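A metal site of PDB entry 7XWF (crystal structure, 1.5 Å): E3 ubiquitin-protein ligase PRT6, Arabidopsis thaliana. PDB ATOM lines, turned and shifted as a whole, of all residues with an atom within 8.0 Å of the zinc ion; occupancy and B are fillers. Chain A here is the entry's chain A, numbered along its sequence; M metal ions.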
ATOM      1  N   ARG A  21       1.791 -21.095 -12.755  1.00  0.00           N
ATOM      2  CA  ARG A  21       1.109 -20.184 -13.635  1.00  0.00           C
ATOM      3  C   ARG A  21       1.337 -20.668 -15.062  1.00  0.00           C
ATOM      4  O   ARG A  21       2.450 -21.024 -15.428  1.00  0.00           O
ATOM      5  CB  ARG A  21       1.686 -18.774 -13.473  1.00  0.00           C
ATOM      6  CG  ARG A  21       1.129 -17.804 -14.521  1.00  0.00           C
ATOM      7  CD  ARG A  21       1.355 -16.344 -14.205  1.00  0.00           C
ATOM      8  NE  ARG A  21       0.544 -15.501 -15.089  1.00  0.00           N
ATOM      9  CZ  ARG A  21       0.813 -14.240 -15.342  1.00  0.00           C
ATOM     10  NH1 ARG A  21       1.863 -13.660 -14.774  1.00  0.00           N
ATOM     11  NH2 ARG A  21       0.039 -13.572 -16.178  1.00  0.00           N
ATOM     12  N   CYS A  22       0.280 -20.670 -15.881  1.00  0.00           N
ATOM     13  CA  CYS A  22       0.467 -20.913 -17.303  1.00  0.00           C
ATOM     14  C   CYS A  22      -0.190 -19.780 -18.065  1.00  0.00           C
ATOM     15  O   CYS A  22      -1.414 -19.704 -18.137  1.00  0.00           O
ATOM     16  CB  CYS A  22      -0.074 -22.262 -17.797  1.00  0.00           C
ATOM     17  SG  CYS A  22       0.404 -22.447 -19.542  1.00  0.00           S
ATOM     18  N   ARG A  23       0.616 -18.889 -18.661  1.00  0.00           N
ATOM     19  CA  ARG A  23       0.038 -17.733 -19.337  1.00  0.00           C
ATOM     20  C   ARG A  23      -0.682 -18.115 -20.610  1.00  0.00           C
ATOM     21  O   ARG A  23      -1.522 -17.341 -21.098  1.00  0.00           O
ATOM     22  CB  ARG A  23       1.156 -16.746 -19.638  1.00  0.00           C
ATOM     23  CG  ARG A  23       1.786 -16.199 -18.390  1.00  0.00           C
ATOM     24  CD  ARG A  23       3.115 -15.553 -18.660  1.00  0.00           C
ATOM     25  NE  ARG A  23       3.832 -15.180 -17.436  1.00  0.00           N
ATOM     26  CZ  ARG A  23       4.524 -16.038 -16.675  1.00  0.00           C
ATOM     27  NH1 ARG A  23       4.592 -17.313 -16.993  1.00  0.00           N
ATOM     28  NH2 ARG A  23       5.153 -15.599 -15.599  1.00  0.00           N
ATOM     29  N   THR A  24      -0.370 -19.274 -21.183  1.00  0.00           N
ATOM     30  CA  THR A  24      -1.108 -19.732 -22.348  1.00  0.00           C
ATOM     31  C   THR A  24      -2.517 -20.212 -21.989  1.00  0.00           C
ATOM     32  O   THR A  24      -3.448 -20.057 -22.781  1.00  0.00           O
ATOM     33  CB  THR A  24      -0.323 -20.875 -22.991  1.00  0.00           C
ATOM     34  OG1 THR A  24       1.036 -20.456 -23.202  1.00  0.00           O
ATOM     35  CG2 THR A  24      -0.936 -21.275 -24.323  1.00  0.00           C
ATOM     36  N   CYS A  25      -2.692 -20.792 -20.812  1.00  0.00           N
ATOM     37  CA  CYS A  25      -3.943 -21.444 -20.446  1.00  0.00           C
ATOM     38  C   CYS A  25      -4.820 -20.624 -19.516  1.00  0.00           C
ATOM     39  O   CYS A  25      -6.030 -20.866 -19.463  1.00  0.00           O
ATOM     40  CB  CYS A  25      -3.673 -22.815 -19.764  1.00  0.00           C
ATOM     41  SG  CYS A  25      -2.982 -24.079 -20.829  1.00  0.00           S
ATOM     42  N   GLU A  26      -4.261 -19.640 -18.815  1.00  0.00           N
ATOM     43  CA  GLU A  26      -5.007 -18.950 -17.776  1.00  0.00           C
ATOM     44  C   GLU A  26      -6.138 -18.112 -18.393  1.00  0.00           C
ATOM     45  O   GLU A  26      -6.036 -17.587 -19.505  1.00  0.00           O
ATOM     46  CB  GLU A  26      -4.035 -18.064 -16.999  1.00  0.00           C
ATOM     47  CG  GLU A  26      -3.531 -16.887 -17.773  1.00  0.00           C
ATOM     48  CD  GLU A  26      -2.427 -16.116 -17.074  1.00  0.00           C
ATOM     49  OE1 GLU A  26      -1.760 -16.675 -16.185  1.00  0.00           O
ATOM     50  OE2 GLU A  26      -2.210 -14.936 -17.450  1.00  0.00           O
ATOM     51  N   ILE A  33      -2.724 -23.422 -11.489  1.00  0.00           N
ATOM     52  CA  ILE A  33      -3.060 -24.817 -11.267  1.00  0.00           C
ATOM     53  C   ILE A  33      -1.991 -25.484 -10.407  1.00  0.00           C
ATOM     54  O   ILE A  33      -0.823 -25.098 -10.405  1.00  0.00           O
ATOM     55  CB  ILE A  33      -3.331 -25.627 -12.536  1.00  0.00           C
ATOM     56  CG1 ILE A  33      -2.134 -25.610 -13.462  1.00  0.00           C
ATOM     57  CG2 ILE A  33      -4.593 -25.075 -13.213  1.00  0.00           C
ATOM     58  CD1 ILE A  33      -2.312 -26.560 -14.658  1.00  0.00           C
ATOM     59  N   PHE A  38      -0.749 -29.671 -13.335  1.00  0.00           N
ATOM     60  CA  PHE A  38       0.189 -29.292 -14.373  1.00  0.00           C
ATOM     61  C   PHE A  38       0.851 -30.508 -15.013  1.00  0.00           C
ATOM     62  O   PHE A  38       0.949 -30.609 -16.235  1.00  0.00           O
ATOM     63  CB  PHE A  38       1.233 -28.331 -13.827  1.00  0.00           C
ATOM     64  CG  PHE A  38       2.187 -27.846 -14.874  1.00  0.00           C
ATOM     65  CD1 PHE A  38       1.851 -26.759 -15.671  1.00  0.00           C
ATOM     66  CD2 PHE A  38       3.415 -28.475 -15.090  1.00  0.00           C
ATOM     67  CE1 PHE A  38       2.728 -26.306 -16.645  1.00  0.00           C
ATOM     68  CE2 PHE A  38       4.278 -28.023 -16.069  1.00  0.00           C
ATOM     69  CZ  PHE A  38       3.939 -26.940 -16.837  1.00  0.00           C
ATOM     70  N   GLY A  41      -1.247 -32.652 -17.494  1.00  0.00           N
ATOM     71  CA  GLY A  41      -1.778 -32.000 -18.670  1.00  0.00           C
ATOM     72  C   GLY A  41      -0.664 -31.726 -19.664  1.00  0.00           C
ATOM     73  O   GLY A  41       0.485 -32.137 -19.465  1.00  0.00           O
ATOM     74  N   ASP A  42      -0.987 -31.012 -20.741  1.00  0.00           N
ATOM     75  CA  ASP A  42      -0.040 -30.767 -21.828  1.00  0.00           C
ATOM     76  C   ASP A  42       0.225 -29.267 -21.909  1.00  0.00           C
ATOM     77  O   ASP A  42      -0.620 -28.523 -22.415  1.00  0.00           O
ATOM     78  CB  ASP A  42      -0.616 -31.302 -23.144  1.00  0.00           C
ATOM     79  CG  ASP A  42       0.338 -31.138 -24.327  1.00  0.00           C
ATOM     80  OD1 ASP A  42       0.058 -31.741 -25.385  1.00  0.00           O
ATOM     81  OD2 ASP A  42       1.353 -30.409 -24.208  1.00  0.00           O
ATOM     82  N   HIS A  43       1.396 -28.838 -21.422  1.00  0.00           N
ATOM     83  CA  HIS A  43       1.819 -27.446 -21.493  1.00  0.00           C
ATOM     84  C   HIS A  43       3.139 -27.313 -22.253  1.00  0.00           C
ATOM     85  O   HIS A  43       3.850 -26.315 -22.080  1.00  0.00           O
ATOM     86  CB  HIS A  43       1.863 -26.821 -20.097  1.00  0.00           C
ATOM     87  CG  HIS A  43       0.559 -26.955 -19.382  1.00  0.00           C
ATOM     88  ND1 HIS A  43      -0.476 -26.052 -19.545  1.00  0.00           N
ATOM     89  CD2 HIS A  43       0.098 -27.935 -18.571  1.00  0.00           C
ATOM     90  CE1 HIS A  43      -1.525 -26.481 -18.845  1.00  0.00           C
ATOM     91  NE2 HIS A  43      -1.197 -27.607 -18.239  1.00  0.00           N
ATOM     92  N   ASN A  44       3.452 -28.288 -23.096  1.00  0.00           N
ATOM     93  CA  ASN A  44       4.597 -28.198 -23.983  1.00  0.00           C
ATOM     94  C   ASN A  44       4.455 -26.966 -24.849  1.00  0.00           C
ATOM     95  O   ASN A  44       3.418 -26.736 -25.478  1.00  0.00           O
ATOM     96  CB  ASN A  44       4.635 -29.441 -24.872  1.00  0.00           C
ATOM     97  CG  ASN A  44       4.856 -30.740 -24.079  1.00  0.00           C
ATOM     98  OD1 ASN A  44       4.301 -31.791 -24.411  1.00  0.00           O
ATOM     99  ND2 ASN A  44       5.675 -30.646 -23.033  1.00  0.00           N
ATOM    100  N   SER A  45       5.510 -26.149 -24.878  1.00  0.00           N
ATOM    101  CA  SER A  45       5.564 -24.920 -25.639  1.00  0.00           C
ATOM    102  C   SER A  45       4.767 -23.795 -25.000  1.00  0.00           C
ATOM    103  O   SER A  45       4.681 -22.719 -25.593  1.00  0.00           O
ATOM    104  CB  SER A  45       5.054 -25.091 -27.082  1.00  0.00           C
ATOM    105  OG  SER A  45       3.656 -24.855 -27.158  1.00  0.00           O
ATOM    106  N   HIS A  46       4.144 -23.999 -23.839  1.00  0.00           N
ATOM    107  CA  HIS A  46       3.372 -22.947 -23.185  1.00  0.00           C
ATOM    108  C   HIS A  46       4.289 -22.063 -22.363  1.00  0.00           C
ATOM    109  O   HIS A  46       5.410 -22.441 -22.039  1.00  0.00           O
ATOM    110  CB  HIS A  46       2.320 -23.549 -22.251  1.00  0.00           C
ATOM    111  CG  HIS A  46       1.199 -24.241 -22.966  1.00  0.00           C
ATOM    112  ND1 HIS A  46       0.021 -24.532 -22.341  1.00  0.00           N
ATOM    113  CD2 HIS A  46       1.103 -24.718 -24.220  1.00  0.00           C
ATOM    114  CE1 HIS A  46      -0.798 -25.132 -23.197  1.00  0.00           C
ATOM    115  NE2 HIS A  46      -0.148 -25.273 -24.341  1.00  0.00           N
ATOM    116  N   ASP A  47       3.808 -20.860 -22.038  1.00  0.00           N
ATOM    117  CA  ASP A  47       4.624 -19.928 -21.261  1.00  0.00           C
ATOM    118  C   ASP A  47       4.267 -20.037 -19.782  1.00  0.00           C
ATOM    119  O   ASP A  47       3.494 -19.252 -19.240  1.00  0.00           O
ATOM    120  CB  ASP A  47       4.495 -18.509 -21.768  1.00  0.00           C
ATOM    121  CG  ASP A  47       5.457 -17.570 -21.079  1.00  0.00           C
ATOM    122  OD1 ASP A  47       6.306 -18.073 -20.301  1.00  0.00           O
ATOM    123  OD2 ASP A  47       5.369 -16.347 -21.300  1.00  0.00           O
ATOM    124  N   TYR A  48       4.798 -21.065 -19.135  1.00  0.00           N
ATOM    125  CA  TYR A  48       4.469 -21.391 -17.755  1.00  0.00           C
ATOM    126  C   TYR A  48       5.641 -21.074 -16.838  1.00  0.00           C
ATOM    127  O   TYR A  48       6.808 -21.016 -17.253  1.00  0.00           O
ATOM    128  CB  TYR A  48       4.048 -22.860 -17.608  1.00  0.00           C
ATOM    129  CG  TYR A  48       5.107 -23.849 -18.033  1.00  0.00           C
ATOM    130  CD1 TYR A  48       6.104 -24.220 -17.158  1.00  0.00           C
ATOM    131  CD2 TYR A  48       5.101 -24.407 -19.302  1.00  0.00           C
ATOM    132  CE1 TYR A  48       7.090 -25.108 -17.534  1.00  0.00           C
ATOM    133  CE2 TYR A  48       6.098 -25.295 -19.687  1.00  0.00           C
ATOM    134  CZ  TYR A  48       7.084 -25.648 -18.791  1.00  0.00           C
ATOM    135  OH  TYR A  48       8.061 -26.535 -19.144  1.00  0.00           O
ATOM    136  N   TRP A  66      -9.819 -21.303 -16.461  1.00  0.00           N
ATOM    137  CA  TRP A  66      -8.744 -21.996 -17.143  1.00  0.00           C
ATOM    138  C   TRP A  66      -9.265 -22.550 -18.460  1.00  0.00           C
ATOM    139  O   TRP A  66     -10.382 -23.092 -18.517  1.00  0.00           O
ATOM    140  CB  TRP A  66      -8.224 -23.105 -16.246  1.00  0.00           C
ATOM    141  CG  TRP A  66      -6.860 -23.610 -16.513  1.00  0.00           C
ATOM    142  CD1 TRP A  66      -6.520 -24.759 -17.163  1.00  0.00           C
ATOM    143  CD2 TRP A  66      -5.626 -23.027 -16.054  1.00  0.00           C
ATOM    144  NE1 TRP A  66      -5.148 -24.908 -17.182  1.00  0.00           N
ATOM    145  CE2 TRP A  66      -4.578 -23.850 -16.509  1.00  0.00           C
ATOM    146  CE3 TRP A  66      -5.312 -21.870 -15.331  1.00  0.00           C
ATOM    147  CZ2 TRP A  66      -3.239 -23.581 -16.226  1.00  0.00           C
ATOM    148  CZ3 TRP A  66      -3.980 -21.586 -15.091  1.00  0.00           C
ATOM    149  CH2 TRP A  66      -2.963 -22.435 -15.539  1.00  0.00           C
ATOM    150  N   LYS A  67      -8.455 -22.448 -19.509  1.00  0.00           N
ATOM    151  CA  LYS A  67      -8.868 -22.895 -20.834  1.00  0.00           C
ATOM    152  C   LYS A  67      -8.967 -24.428 -20.843  1.00  0.00           C
ATOM    153  O   LYS A  67      -8.057 -25.109 -20.344  1.00  0.00           O
ATOM    154  CB  LYS A  67      -7.907 -22.394 -21.904  1.00  0.00           C
ATOM    155  CG  LYS A  67      -7.955 -20.876 -22.086  1.00  0.00           C
ATOM    156  CD  LYS A  67      -6.839 -20.378 -23.002  1.00  0.00           C
ATOM    157  CE  LYS A  67      -6.692 -18.856 -22.935  1.00  0.00           C
ATOM    158  NZ  LYS A  67      -5.602 -18.381 -23.817  1.00  0.00           N
ATOM    159  N   ASP A  69      -8.384 -26.790 -22.912  1.00  0.00           N
ATOM    160  CA  ASP A  69      -7.280 -27.561 -23.451  1.00  0.00           C
ATOM    161  C   ASP A  69      -6.110 -27.652 -22.465  1.00  0.00           C
ATOM    162  O   ASP A  69      -5.214 -28.469 -22.680  1.00  0.00           O
ATOM    163  CB  ASP A  69      -6.813 -26.996 -24.797  1.00  0.00           C
ATOM    164  CG  ASP A  69      -6.365 -25.549 -24.724  1.00  0.00           C
ATOM    165  OD1 ASP A  69      -7.260 -24.669 -24.750  1.00  0.00           O
ATOM    166  OD2 ASP A  69      -5.140 -25.294 -24.659  1.00  0.00           O
ATOM    167  N   GLY A  70      -6.106 -26.816 -21.420  1.00  0.00           N
ATOM    168  CA  GLY A  70      -5.143 -26.872 -20.338  1.00  0.00           C
ATOM    169  C   GLY A  70      -5.552 -27.689 -19.143  1.00  0.00           C
ATOM    170  O   GLY A  70      -4.804 -27.696 -18.144  1.00  0.00           O
ATOM    171  N   PHE A  71      -6.683 -28.389 -19.203  1.00  0.00           N
ATOM    172  CA  PHE A  71      -7.089 -29.270 -18.120  1.00  0.00           C
ATOM    173  C   PHE A  71      -6.233 -30.526 -18.136  1.00  0.00           C
ATOM    174  O   PHE A  71      -5.753 -30.977 -19.175  1.00  0.00           O
ATOM    175  CB  PHE A  71      -8.544 -29.729 -18.329  1.00  0.00           C
ATOM    176  CG  PHE A  71      -9.583 -28.652 -18.143  1.00  0.00           C
ATOM    177  CD1 PHE A  71     -10.911 -28.931 -18.413  1.00  0.00           C
ATOM    178  CD2 PHE A  71      -9.250 -27.369 -17.704  1.00  0.00           C
ATOM    179  CE1 PHE A  71     -11.897 -27.974 -18.257  1.00  0.00           C
ATOM    180  CE2 PHE A  71     -10.234 -26.411 -17.534  1.00  0.00           C
ATOM    181  CZ  PHE A  71     -11.561 -26.707 -17.803  1.00  0.00           C
HETATM  182 ZN    ZN M   1      -0.715 -24.221 -20.448  1.00  0.00          ZN
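The side-chain sulfur (SG) of Cys 22 sits close to the backbone NH (N) of Thr 24, 3.7 Å away. O of Cys 25 sits at hydrogen-bond distance from N of Lys 67, at 2.9 Å.
Within 4 Å of the zinc ion: Cys 22, Cys 25, His 43 and His 46. The nearest printed residue that does not touch the zinc ion is Thr 24 (4.2 Å).
The zinc ion is bound by a ring nitrogen (ND1) of His 46 (2.1 Å), a ring nitrogen (ND1) of His 43 (2.1 Å), the side-chain sulfur of Cys 22 (2.3 Å) and the side-chain sulfur of Cys 25 (2.3 Å). The zinc ion has four donor atoms within binding distance.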
